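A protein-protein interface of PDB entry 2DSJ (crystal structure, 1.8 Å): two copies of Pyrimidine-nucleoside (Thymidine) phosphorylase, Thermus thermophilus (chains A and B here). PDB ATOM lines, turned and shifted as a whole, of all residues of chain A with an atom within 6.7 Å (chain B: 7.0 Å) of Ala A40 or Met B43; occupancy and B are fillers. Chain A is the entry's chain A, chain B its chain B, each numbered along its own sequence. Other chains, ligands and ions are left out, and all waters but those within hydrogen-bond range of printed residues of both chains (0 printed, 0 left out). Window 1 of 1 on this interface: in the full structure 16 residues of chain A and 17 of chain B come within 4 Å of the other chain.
Among the printed residues, pairs that only touch across the chains: Arg A11 with Phe B46 (3.3 Å), Ile A7 with Met B43 (3.5 Å), Arg A11 with Leu B47 (3.5 Å), Met A43 with Ala B40 (3.5 Å), Ala A40 with Met B43 (3.6 Å), Ile A7 with Thr B170 (3.6 Å), Arg A11 with Met B43 (3.7 Å), Tyr A36 with Val B169 (3.7 Å), Tyr A36 with Tyr B36 (3.7 Å), Asp A35 with Tyr B36 (3.7 Å), Met A43 with Ala B44 (3.7 Å), Met A43 with Met B43 (3.7 Å), Leu A47 with Leu B47 (3.7 Å), Tyr A36 with Thr B170 (3.8 Å), Ala A44 with Met B43 (3.8 Å), Arg A8 with Ala B171 (3.8 Å), Ile A7 with Ala B171 (3.9 Å), Ser A39 with Ala B40 (3.99 Å) and Ala A40 with Thr B170 (3.99 Å).
Tyr A36 touches Ser B39, and with the chains exchanged Ser A39 touches Tyr B36.
Ala A40 touches Met B43, and with the chains exchanged Met A43 touches Ala B40.
Met A43 touches its own counterpart, Met B43.
Leu A47 touches its own counterpart, Leu B47.
Of the 24 pairs that touch across the chains among the printed residues, 10 have their exchanged pair printed and touching as well.
Hydrophobic or aromatic side chains of chain B that line the printed part of chain A: Tyr B36, Met B43, Phe B46, Leu B47, Val B169 and Ala B171.
Of the 17 printed residues of chain A, 11 touch a printed residue of chain B.
Hydrophobic or aromatic side chains of chain A within 4 Å of the printed part of chain B: Ile A7, Tyr A36, Ala A40, Met A43 and Leu A47.
Along chain A the printed residues that touch a printed residue of chain B span positions 7 to 47.
Printed residues of chain B within 4 Å of Arg A11: Met B43, Phe B46, Leu B47 and Ala B171.
Of the printed residues of chain B, Ala A40 touches Met B43 (3.6 Å) and Thr B170 (3.99 Å).
Of the printed residues of chain B, Met A43 touches Ala B40 (3.5 Å), Met B43 (3.7 Å) and Ala B44 (3.7 Å).
Of the printed residues of chain A, Met B43 touches Ile A7 (3.5 Å), Arg A11 (3.7 Å), Ala A40 (3.6 Å), Met A43 (3.7 Å) and Ala A44 (3.8 Å).
Printed residues of chain A within 4 Å of Ala B44: Met A43.
Ala B45 touches none of the printed residues of chain A.
Printed residues of chain A within 4 Å of Leu B47: Arg A11 and Leu A47.
Arg B48 touches none of the printed residues of chain A.
The nearest residue of chain A that does not touch Met B43 is Leu A47 (4.6 Å).
OG of Ser A39 lies within hydrogen-bond range of O of Asp A35.
OG of Ser A39 is in hydrogen-bond range of O of Tyr A36 (3.2 Å).
The side-chain hydroxyl (OG) of Ser B39 is in hydrogen-bond range of the backbone carbonyl oxygen (O) of Tyr B36.
The side-chain hydroxyl (OG1) of Thr B172 is in hydrogen-bond range of the side-chain hydroxyl (OG1) of Thr B170 (2.7 Å).
NH1 of Arg A11 is in hydrogen-bond range of O of Ala B171 (2.8 Å).
O of Tyr A36 lies within hydrogen-bond range of OG of Ser B39 (2.8 Å).
The backbone carbonyl oxygen (O) of Val B169 lies within hydrogen-bond range of the side-chain amide nitrogen (NE2) of Gln A37 (2.9 Å).
The backbone carbonyl oxygen of Tyr B36 is in hydrogen-bond range of the side-chain hydroxyl of Ser A39 (2.8 Å).
The side-chain hydroxyl (OG) of Ser A39 lies within hydrogen-bond range of the side-chain hydroxyl (OG) of Ser B39, 2.7 Å away.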
ATOM      1  N   ILE A   7     -29.079 -16.855  10.321  1.00  0.00           N
ATOM      2  CA  ILE A   7     -28.434 -17.436  11.500  1.00  0.00           C
ATOM      3  C   ILE A   7     -26.917 -17.480  11.281  1.00  0.00           C
ATOM      4  O   ILE A   7     -26.141 -17.038  12.130  1.00  0.00           O
ATOM      5  CB  ILE A   7     -28.929 -18.880  11.759  1.00  0.00           C
ATOM      6  CG1 ILE A   7     -30.440 -18.889  11.992  1.00  0.00           C
ATOM      7  CG2 ILE A   7     -28.190 -19.486  12.955  1.00  0.00           C
ATOM      8  CD1 ILE A   7     -31.051 -20.290  11.940  1.00  0.00           C
ATOM      9  N   ARG A   8     -26.498 -18.011  10.133  1.00  0.00           N
ATOM     10  CA  ARG A   8     -25.071 -18.117   9.825  1.00  0.00           C
ATOM     11  C   ARG A   8     -24.361 -16.776   9.864  1.00  0.00           C
ATOM     12  O   ARG A   8     -23.233 -16.675  10.344  1.00  0.00           O
ATOM     13  CB  ARG A   8     -24.857 -18.762   8.450  1.00  0.00           C
ATOM     14  CG  ARG A   8     -23.388 -18.948   8.088  1.00  0.00           C
ATOM     15  CD  ARG A   8     -23.228 -19.742   6.797  1.00  0.00           C
ATOM     16  NE  ARG A   8     -23.776 -21.087   6.931  1.00  0.00           N
ATOM     17  CZ  ARG A   8     -24.801 -21.554   6.225  1.00  0.00           C
ATOM     18  NH1 ARG A   8     -25.394 -20.782   5.322  1.00  0.00           N
ATOM     19  NH2 ARG A   8     -25.245 -22.787   6.433  1.00  0.00           N
ATOM     20  N   LYS A  10     -24.904 -14.195  11.717  1.00  0.00           N
ATOM     21  CA  LYS A  10     -24.580 -13.819  13.091  1.00  0.00           C
ATOM     22  C   LYS A  10     -23.579 -14.804  13.702  1.00  0.00           C
ATOM     23  O   LYS A  10     -22.696 -14.404  14.453  1.00  0.00           O
ATOM     24  CB  LYS A  10     -25.862 -13.740  13.933  1.00  0.00           C
ATOM     25  CG  LYS A  10     -25.655 -13.291  15.388  1.00  0.00           C
ATOM     26  CD  LYS A  10     -24.866 -11.990  15.506  1.00  0.00           C
ATOM     27  CE  LYS A  10     -25.535 -10.834  14.768  1.00  0.00           C
ATOM     28  NZ  LYS A  10     -24.750  -9.571  14.936  1.00  0.00           N
ATOM     29  N   ARG A  11     -23.706 -16.083  13.360  1.00  0.00           N
ATOM     30  CA  ARG A  11     -22.797 -17.109  13.870  1.00  0.00           C
ATOM     31  C   ARG A  11     -21.358 -16.702  13.573  1.00  0.00           C
ATOM     32  O   ARG A  11     -20.448 -16.946  14.372  1.00  0.00           O
ATOM     33  CB  ARG A  11     -23.095 -18.453  13.199  1.00  0.00           C
ATOM     34  CG  ARG A  11     -22.268 -19.614  13.722  1.00  0.00           C
ATOM     35  CD  ARG A  11     -22.311 -20.785  12.754  1.00  0.00           C
ATOM     36  NE  ARG A  11     -21.463 -20.560  11.582  1.00  0.00           N
ATOM     37  CZ  ARG A  11     -21.463 -21.334  10.498  1.00  0.00           C
ATOM     38  NH1 ARG A  11     -22.271 -22.380  10.427  1.00  0.00           N
ATOM     39  NH2 ARG A  11     -20.637 -21.071   9.490  1.00  0.00           N
ATOM     40  N   ASP A  35     -39.323 -22.235  15.882  1.00  0.00           N
ATOM     41  CA  ASP A  35     -38.653 -21.863  17.119  1.00  0.00           C
ATOM     42  C   ASP A  35     -37.200 -22.334  17.160  1.00  0.00           C
ATOM     43  O   ASP A  35     -36.359 -21.689  17.785  1.00  0.00           O
ATOM     44  CB  ASP A  35     -39.386 -22.421  18.349  1.00  0.00           C
ATOM     45  CG  ASP A  35     -40.798 -21.880  18.489  1.00  0.00           C
ATOM     46  OD1 ASP A  35     -41.018 -20.701  18.156  1.00  0.00           O
ATOM     47  OD2 ASP A  35     -41.686 -22.630  18.949  1.00  0.00           O
ATOM     48  N   TYR A  36     -36.894 -23.454  16.506  1.00  0.00           N
ATOM     49  CA  TYR A  36     -35.520 -23.953  16.536  1.00  0.00           C
ATOM     50  C   TYR A  36     -34.540 -23.115  15.710  1.00  0.00           C
ATOM     51  O   TYR A  36     -33.332 -23.135  15.962  1.00  0.00           O
ATOM     52  CB  TYR A  36     -35.472 -25.437  16.129  1.00  0.00           C
ATOM     53  CG  TYR A  36     -35.998 -25.745  14.749  1.00  0.00           C
ATOM     54  CD1 TYR A  36     -35.268 -25.405  13.612  1.00  0.00           C
ATOM     55  CD2 TYR A  36     -37.222 -26.398  14.579  1.00  0.00           C
ATOM     56  CE1 TYR A  36     -35.737 -25.709  12.338  1.00  0.00           C
ATOM     57  CE2 TYR A  36     -37.702 -26.706  13.305  1.00  0.00           C
ATOM     58  CZ  TYR A  36     -36.954 -26.359  12.192  1.00  0.00           C
ATOM     59  OH  TYR A  36     -37.416 -26.655  10.930  1.00  0.00           O
ATOM     60  N   GLN A  37     -35.035 -22.373  14.727  1.00  0.00           N
ATOM     61  CA  GLN A  37     -34.137 -21.526  13.954  1.00  0.00           C
ATOM     62  C   GLN A  37     -33.938 -20.225  14.726  1.00  0.00           C
ATOM     63  O   GLN A  37     -32.864 -19.632  14.701  1.00  0.00           O
ATOM     64  CB  GLN A  37     -34.695 -21.231  12.560  1.00  0.00           C
ATOM     65  CG  GLN A  37     -34.679 -22.439  11.627  1.00  0.00           C
ATOM     66  CD  GLN A  37     -34.971 -22.078  10.184  1.00  0.00           C
ATOM     67  OE1 GLN A  37     -35.882 -21.300   9.898  1.00  0.00           O
ATOM     68  NE2 GLN A  37     -34.203 -22.654   9.260  1.00  0.00           N
ATOM     69  N   VAL A  38     -34.976 -19.787  15.428  1.00  0.00           N
ATOM     70  CA  VAL A  38     -34.862 -18.558  16.204  1.00  0.00           C
ATOM     71  C   VAL A  38     -33.967 -18.783  17.422  1.00  0.00           C
ATOM     72  O   VAL A  38     -33.209 -17.895  17.803  1.00  0.00           O
ATOM     73  CB  VAL A  38     -36.241 -18.049  16.681  1.00  0.00           C
ATOM     74  CG1 VAL A  38     -36.065 -16.769  17.506  1.00  0.00           C
ATOM     75  CG2 VAL A  38     -37.134 -17.787  15.482  1.00  0.00           C
ATOM     76  N   SER A  39     -34.047 -19.963  18.031  1.00  0.00           N
ATOM     77  CA  SER A  39     -33.214 -20.246  19.200  1.00  0.00           C
ATOM     78  C   SER A  39     -31.745 -20.337  18.789  1.00  0.00           C
ATOM     79  O   SER A  39     -30.857 -19.957  19.549  1.00  0.00           O
ATOM     80  CB  SER A  39     -33.642 -21.543  19.893  1.00  0.00           C
ATOM     81  OG  SER A  39     -33.417 -22.681  19.080  1.00  0.00           O
ATOM     82  N   ALA A  40     -31.494 -20.855  17.591  1.00  0.00           N
ATOM     83  CA  ALA A  40     -30.130 -20.953  17.093  1.00  0.00           C
ATOM     84  C   ALA A  40     -29.611 -19.534  16.891  1.00  0.00           C
ATOM     85  O   ALA A  40     -28.468 -19.228  17.238  1.00  0.00           O
ATOM     86  CB  ALA A  40     -30.097 -21.725  15.766  1.00  0.00           C
ATOM     87  N   TRP A  41     -30.447 -18.662  16.327  1.00  0.00           N
ATOM     88  CA  TRP A  41     -30.029 -17.280  16.116  1.00  0.00           C
ATOM     89  C   TRP A  41     -29.805 -16.577  17.454  1.00  0.00           C
ATOM     90  O   TRP A  41     -28.845 -15.823  17.611  1.00  0.00           O
ATOM     91  CB  TRP A  41     -31.068 -16.491  15.316  1.00  0.00           C
ATOM     92  CG  TRP A  41     -30.696 -15.042  15.214  1.00  0.00           C
ATOM     93  CD1 TRP A  41     -29.702 -14.501  14.452  1.00  0.00           C
ATOM     94  CD2 TRP A  41     -31.250 -13.963  15.978  1.00  0.00           C
ATOM     95  NE1 TRP A  41     -29.598 -13.150  14.698  1.00  0.00           N
ATOM     96  CE2 TRP A  41     -30.537 -12.796  15.629  1.00  0.00           C
ATOM     97  CE3 TRP A  41     -32.279 -13.871  16.929  1.00  0.00           C
ATOM     98  CZ2 TRP A  41     -30.818 -11.547  16.197  1.00  0.00           C
ATOM     99  CZ3 TRP A  41     -32.558 -12.628  17.492  1.00  0.00           C
ATOM    100  CH2 TRP A  41     -31.829 -11.485  17.123  1.00  0.00           C
ATOM    101  N   LEU A  42     -30.695 -16.813  18.411  1.00  0.00           N
ATOM    102  CA  LEU A  42     -30.558 -16.188  19.730  1.00  0.00           C
ATOM    103  C   LEU A  42     -29.238 -16.573  20.393  1.00  0.00           C
ATOM    104  O   LEU A  42     -28.593 -15.741  21.028  1.00  0.00           O
ATOM    105  CB  LEU A  42     -31.721 -16.592  20.642  1.00  0.00           C
ATOM    106  CG  LEU A  42     -33.061 -15.901  20.384  1.00  0.00           C
ATOM    107  CD1 LEU A  42     -34.173 -16.657  21.110  1.00  0.00           C
ATOM    108  CD2 LEU A  42     -32.992 -14.454  20.860  1.00  0.00           C
ATOM    109  N   MET A  43     -28.835 -17.833  20.250  1.00  0.00           N
ATOM    110  CA  MET A  43     -27.583 -18.281  20.849  1.00  0.00           C
ATOM    111  C   MET A  43     -26.399 -17.610  20.157  1.00  0.00           C
ATOM    112  O   MET A  43     -25.410 -17.267  20.803  1.00  0.00           O
ATOM    113  CB  MET A  43     -27.451 -19.802  20.753  1.00  0.00           C
ATOM    114  CG  MET A  43     -26.224 -20.365  21.463  1.00  0.00           C
ATOM    115  SD  MET A  43     -26.121 -19.843  23.211  1.00  0.00           S
ATOM    116  CE  MET A  43     -27.318 -20.977  23.985  1.00  0.00           C
ATOM    117  N   ALA A  44     -26.498 -17.431  18.843  1.00  0.00           N
ATOM    118  CA  ALA A  44     -25.433 -16.779  18.089  1.00  0.00           C
ATOM    119  C   ALA A  44     -25.370 -15.301  18.488  1.00  0.00           C
ATOM    120  O   ALA A  44     -24.289 -14.745  18.671  1.00  0.00           O
ATOM    121  CB  ALA A  44     -25.690 -16.917  16.593  1.00  0.00           C
ATOM    122  N   ALA A  45     -26.533 -14.669  18.629  1.00  0.00           N
ATOM    123  CA  ALA A  45     -26.573 -13.263  19.020  1.00  0.00           C
ATOM    124  C   ALA A  45     -26.011 -13.110  20.432  1.00  0.00           C
ATOM    125  O   ALA A  45     -25.293 -12.158  20.730  1.00  0.00           O
ATOM    126  CB  ALA A  45     -28.006 -12.740  18.965  1.00  0.00           C
ATOM    127  N   LEU A  47     -23.796 -15.057  21.932  1.00  0.00           N
ATOM    128  CA  LEU A  47     -22.353 -15.276  21.908  1.00  0.00           C
ATOM    129  C   LEU A  47     -21.507 -14.366  21.018  1.00  0.00           C
ATOM    130  O   LEU A  47     -20.361 -14.070  21.360  1.00  0.00           O
ATOM    131  CB  LEU A  47     -22.068 -16.739  21.560  1.00  0.00           C
ATOM    132  CG  LEU A  47     -22.484 -17.719  22.661  1.00  0.00           C
ATOM    133  CD1 LEU A  47     -22.292 -19.152  22.186  1.00  0.00           C
ATOM    134  CD2 LEU A  47     -21.654 -17.452  23.920  1.00  0.00           C
ATOM    135  N   LEU A 166     -39.050 -17.826  24.608  1.00  0.00           N
ATOM    136  CA  LEU A 166     -38.079 -18.714  23.973  1.00  0.00           C
ATOM    137  C   LEU A 166     -36.722 -18.588  24.656  1.00  0.00           C
ATOM    138  O   LEU A 166     -36.076 -19.587  24.950  1.00  0.00           O
ATOM    139  CB  LEU A 166     -37.954 -18.386  22.481  1.00  0.00           C
ATOM    140  CG  LEU A 166     -37.069 -19.321  21.641  1.00  0.00           C
ATOM    141  CD1 LEU A 166     -37.567 -20.757  21.748  1.00  0.00           C
ATOM    142  CD2 LEU A 166     -37.078 -18.856  20.194  1.00  0.00           C
ATOM    143  N   LYS B  10     -22.800 -25.238  28.201  1.00  0.00           N
ATOM    144  CA  LYS B  10     -21.970 -25.144  26.999  1.00  0.00           C
ATOM    145  C   LYS B  10     -21.837 -23.683  26.569  1.00  0.00           C
ATOM    146  O   LYS B  10     -20.782 -23.253  26.108  1.00  0.00           O
ATOM    147  CB  LYS B  10     -22.564 -25.986  25.863  1.00  0.00           C
ATOM    148  CG  LYS B  10     -21.713 -26.009  24.589  1.00  0.00           C
ATOM    149  CD  LYS B  10     -20.239 -26.311  24.883  1.00  0.00           C
ATOM    150  CE  LYS B  10     -20.035 -27.632  25.611  1.00  0.00           C
ATOM    151  NZ  LYS B  10     -18.575 -27.888  25.855  1.00  0.00           N
ATOM    152  N   TYR B  36     -35.877 -26.952  19.549  1.00  0.00           N
ATOM    153  CA  TYR B  36     -35.331 -25.621  19.801  1.00  0.00           C
ATOM    154  C   TYR B  36     -34.311 -25.581  20.945  1.00  0.00           C
ATOM    155  O   TYR B  36     -33.498 -24.659  21.016  1.00  0.00           O
ATOM    156  CB  TYR B  36     -36.456 -24.601  20.040  1.00  0.00           C
ATOM    157  CG  TYR B  36     -37.353 -24.899  21.216  1.00  0.00           C
ATOM    158  CD1 TYR B  36     -36.914 -24.704  22.525  1.00  0.00           C
ATOM    159  CD2 TYR B  36     -38.652 -25.370  21.020  1.00  0.00           C
ATOM    160  CE1 TYR B  36     -37.747 -24.973  23.612  1.00  0.00           C
ATOM    161  CE2 TYR B  36     -39.490 -25.643  22.099  1.00  0.00           C
ATOM    162  CZ  TYR B  36     -39.034 -25.443  23.387  1.00  0.00           C
ATOM    163  OH  TYR B  36     -39.868 -25.716  24.453  1.00  0.00           O
ATOM    164  N   VAL B  38     -32.254 -28.242  21.531  1.00  0.00           N
ATOM    165  CA  VAL B  38     -31.105 -28.930  20.951  1.00  0.00           C
ATOM    166  C   VAL B  38     -30.354 -28.029  19.964  1.00  0.00           C
ATOM    167  O   VAL B  38     -29.124 -28.093  19.874  1.00  0.00           O
ATOM    168  CB  VAL B  38     -31.544 -30.234  20.248  1.00  0.00           C
ATOM    169  CG1 VAL B  38     -30.331 -30.949  19.640  1.00  0.00           C
ATOM    170  CG2 VAL B  38     -32.236 -31.143  21.258  1.00  0.00           C
ATOM    171  N   SER B  39     -31.075 -27.186  19.229  1.00  0.00           N
ATOM    172  CA  SER B  39     -30.413 -26.292  18.283  1.00  0.00           C
ATOM    173  C   SER B  39     -29.666 -25.196  19.033  1.00  0.00           C
ATOM    174  O   SER B  39     -28.616 -24.723  18.584  1.00  0.00           O
ATOM    175  CB  SER B  39     -31.413 -25.675  17.296  1.00  0.00           C
ATOM    176  OG  SER B  39     -32.375 -24.859  17.941  1.00  0.00           O
ATOM    177  N   ALA B  40     -30.211 -24.789  20.177  1.00  0.00           N
ATOM    178  CA  ALA B  40     -29.564 -23.769  20.993  1.00  0.00           C
ATOM    179  C   ALA B  40     -28.248 -24.362  21.487  1.00  0.00           C
ATOM    180  O   ALA B  40     -27.211 -23.698  21.476  1.00  0.00           O
ATOM    181  CB  ALA B  40     -30.459 -23.390  22.173  1.00  0.00           C
ATOM    182  N   TRP B  41     -28.289 -25.623  21.910  1.00  0.00           N
ATOM    183  CA  TRP B  41     -27.079 -26.295  22.376  1.00  0.00           C
ATOM    184  C   TRP B  41     -26.099 -26.485  21.213  1.00  0.00           C
ATOM    185  O   TRP B  41     -24.901 -26.285  21.371  1.00  0.00           O
ATOM    186  CB  TRP B  41     -27.401 -27.662  22.980  1.00  0.00           C
ATOM    187  CG  TRP B  41     -26.157 -28.412  23.354  1.00  0.00           C
ATOM    188  CD1 TRP B  41     -25.338 -28.166  24.420  1.00  0.00           C
ATOM    189  CD2 TRP B  41     -25.542 -29.468  22.609  1.00  0.00           C
ATOM    190  NE1 TRP B  41     -24.244 -29.004  24.379  1.00  0.00           N
ATOM    191  CE2 TRP B  41     -24.347 -29.814  23.279  1.00  0.00           C
ATOM    192  CE3 TRP B  41     -25.884 -30.158  21.437  1.00  0.00           C
ATOM    193  CZ2 TRP B  41     -23.491 -30.819  22.815  1.00  0.00           C
ATOM    194  CZ3 TRP B  41     -25.030 -31.161  20.977  1.00  0.00           C
ATOM    195  CH2 TRP B  41     -23.850 -31.478  21.668  1.00  0.00           C
ATOM    196  N   LEU B  42     -26.612 -26.877  20.047  1.00  0.00           N
ATOM    197  CA  LEU B  42     -25.750 -27.077  18.880  1.00  0.00           C
ATOM    198  C   LEU B  42     -24.974 -25.806  18.552  1.00  0.00           C
ATOM    199  O   LEU B  42     -23.783 -25.859  18.244  1.00  0.00           O
ATOM    200  CB  LEU B  42     -26.580 -27.513  17.667  1.00  0.00           C
ATOM    201  CG  LEU B  42     -26.966 -28.997  17.685  1.00  0.00           C
ATOM    202  CD1 LEU B  42     -28.016 -29.282  16.613  1.00  0.00           C
ATOM    203  CD2 LEU B  42     -25.710 -29.848  17.446  1.00  0.00           C
ATOM    204  N   MET B  43     -25.644 -24.663  18.632  1.00  0.00           N
ATOM    205  CA  MET B  43     -24.985 -23.397  18.341  1.00  0.00           C
ATOM    206  C   MET B  43     -23.943 -23.078  19.413  1.00  0.00           C
ATOM    207  O   MET B  43     -22.874 -22.530  19.113  1.00  0.00           O
ATOM    208  CB  MET B  43     -26.006 -22.260  18.241  1.00  0.00           C
ATOM    209  CG  MET B  43     -25.379 -20.918  17.850  1.00  0.00           C
ATOM    210  SD  MET B  43     -24.540 -20.967  16.243  1.00  0.00           S
ATOM    211  CE  MET B  43     -25.840 -20.842  15.116  1.00  0.00           C
ATOM    212  N   ALA B  44     -24.249 -23.410  20.662  1.00  0.00           N
ATOM    213  CA  ALA B  44     -23.300 -23.176  21.749  1.00  0.00           C
ATOM    214  C   ALA B  44     -22.069 -24.062  21.534  1.00  0.00           C
ATOM    215  O   ALA B  44     -20.933 -23.610  21.694  1.00  0.00           O
ATOM    216  CB  ALA B  44     -23.949 -23.492  23.102  1.00  0.00           C
ATOM    217  N   ALA B  45     -22.292 -25.322  21.162  1.00  0.00           N
ATOM    218  CA  ALA B  45     -21.176 -26.242  20.927  1.00  0.00           C
ATOM    219  C   ALA B  45     -20.344 -25.764  19.738  1.00  0.00           C
ATOM    220  O   ALA B  45     -19.115 -25.866  19.740  1.00  0.00           O
ATOM    221  CB  ALA B  45     -21.696 -27.652  20.661  1.00  0.00           C
ATOM    222  N   PHE B  46     -21.027 -25.248  18.724  1.00  0.00           N
ATOM    223  CA  PHE B  46     -20.371 -24.754  17.522  1.00  0.00           C
ATOM    224  C   PHE B  46     -19.434 -23.600  17.870  1.00  0.00           C
ATOM    225  O   PHE B  46     -18.265 -23.602  17.484  1.00  0.00           O
ATOM    226  CB  PHE B  46     -21.434 -24.280  16.520  1.00  0.00           C
ATOM    227  CG  PHE B  46     -20.896 -23.947  15.152  1.00  0.00           C
ATOM    228  CD1 PHE B  46     -20.028 -22.877  14.965  1.00  0.00           C
ATOM    229  CD2 PHE B  46     -21.280 -24.699  14.044  1.00  0.00           C
ATOM    230  CE1 PHE B  46     -19.548 -22.558  13.694  1.00  0.00           C
ATOM    231  CE2 PHE B  46     -20.807 -24.387  12.772  1.00  0.00           C
ATOM    232  CZ  PHE B  46     -19.936 -23.311  12.600  1.00  0.00           C
ATOM    233  N   LEU B  47     -19.951 -22.626  18.616  1.00  0.00           N
ATOM    234  CA  LEU B  47     -19.172 -21.445  18.982  1.00  0.00           C
ATOM    235  C   LEU B  47     -18.219 -21.578  20.170  1.00  0.00           C
ATOM    236  O   LEU B  47     -17.168 -20.938  20.178  1.00  0.00           O
ATOM    237  CB  LEU B  47     -20.113 -20.260  19.217  1.00  0.00           C
ATOM    238  CG  LEU B  47     -20.880 -19.775  17.983  1.00  0.00           C
ATOM    239  CD1 LEU B  47     -21.910 -18.730  18.392  1.00  0.00           C
ATOM    240  CD2 LEU B  47     -19.905 -19.202  16.956  1.00  0.00           C
ATOM    241  N   ARG B  48     -18.572 -22.383  21.171  1.00  0.00           N
ATOM    242  CA  ARG B  48     -17.700 -22.542  22.338  1.00  0.00           C
ATOM    243  C   ARG B  48     -16.810 -23.774  22.222  1.00  0.00           C
ATOM    244  O   ARG B  48     -15.782 -23.872  22.894  1.00  0.00           O
ATOM    245  CB  ARG B  48     -18.514 -22.618  23.636  1.00  0.00           C
ATOM    246  CG  ARG B  48     -19.353 -21.374  23.953  1.00  0.00           C
ATOM    247  CD  ARG B  48     -18.539 -20.076  23.903  1.00  0.00           C
ATOM    248  NE  ARG B  48     -17.406 -20.060  24.828  1.00  0.00           N
ATOM    249  CZ  ARG B  48     -17.404 -19.481  26.028  1.00  0.00           C
ATOM    250  NH1 ARG B  48     -18.482 -18.856  26.485  1.00  0.00           N
ATOM    251  NH2 ARG B  48     -16.305 -19.510  26.768  1.00  0.00           N
ATOM    252  N   GLY B  49     -17.215 -24.719  21.380  1.00  0.00           N
ATOM    253  CA  GLY B  49     -16.414 -25.913  21.172  1.00  0.00           C
ATOM    254  C   GLY B  49     -16.654 -27.121  22.056  1.00  0.00           C
ATOM    255  O   GLY B  49     -17.273 -27.049  23.120  1.00  0.00           O
ATOM    256  N   VAL B 169     -30.489 -27.286   9.199  1.00  0.00           N
ATOM    257  CA  VAL B 169     -31.434 -26.174   9.109  1.00  0.00           C
ATOM    258  C   VAL B 169     -31.199 -25.105  10.182  1.00  0.00           C
ATOM    259  O   VAL B 169     -32.003 -24.180  10.339  1.00  0.00           O
ATOM    260  CB  VAL B 169     -32.898 -26.671   9.200  1.00  0.00           C
ATOM    261  CG1 VAL B 169     -33.224 -27.544   7.991  1.00  0.00           C
ATOM    262  CG2 VAL B 169     -33.107 -27.456  10.479  1.00  0.00           C
ATOM    263  N   THR B 170     -30.091 -25.230  10.911  1.00  0.00           N
ATOM    264  CA  THR B 170     -29.759 -24.271  11.962  1.00  0.00           C
ATOM    265  C   THR B 170     -28.359 -23.686  11.821  1.00  0.00           C
ATOM    266  O   THR B 170     -27.851 -23.064  12.750  1.00  0.00           O
ATOM    267  CB  THR B 170     -29.860 -24.916  13.354  1.00  0.00           C
ATOM    268  OG1 THR B 170     -28.993 -26.061  13.414  1.00  0.00           O
ATOM    269  CG2 THR B 170     -31.295 -25.342  13.645  1.00  0.00           C
ATOM    270  N   ALA B 171     -27.735 -23.883  10.662  1.00  0.00           N
ATOM    271  CA  ALA B 171     -26.390 -23.372  10.422  1.00  0.00           C
ATOM    272  C   ALA B 171     -25.380 -23.925  11.426  1.00  0.00           C
ATOM    273  O   ALA B 171     -24.488 -23.211  11.887  1.00  0.00           O
ATOM    274  CB  ALA B 171     -26.388 -21.839  10.459  1.00  0.00           C
ATOM    275  N   THR B 172     -25.513 -25.200  11.770  1.00  0.00           N
ATOM    276  CA  THR B 172     -24.571 -25.801  12.707  1.00  0.00           C
ATOM    277  C   THR B 172     -23.897 -27.053  12.142  1.00  0.00           C
ATOM    278  O   THR B 172     -23.482 -27.941  12.883  1.00  0.00           O
ATOM    279  CB  THR B 172     -25.243 -26.114  14.075  1.00  0.00           C
ATOM    280  OG1 THR B 172     -26.474 -26.817  13.876  1.00  0.00           O
ATOM    281  CG2 THR B 172     -25.517 -24.811  14.835  1.00  0.00           C
ATOM    282  N   LEU B 178     -18.511 -31.667  15.228  1.00  0.00           N
ATOM    283  CA  LEU B 178     -19.807 -32.212  14.843  1.00  0.00           C
ATOM    284  C   LEU B 178     -19.711 -33.065  13.578  1.00  0.00           C
ATOM    285  O   LEU B 178     -20.370 -34.098  13.474  1.00  0.00           O
ATOM    286  CB  LEU B 178     -20.829 -31.083  14.653  1.00  0.00           C
ATOM    287  CG  LEU B 178     -21.058 -30.204  15.893  1.00  0.00           C
ATOM    288  CD1 LEU B 178     -22.145 -29.166  15.610  1.00  0.00           C
ATOM    289  CD2 LEU B 178     -21.465 -31.079  17.079  1.00  0.00           C
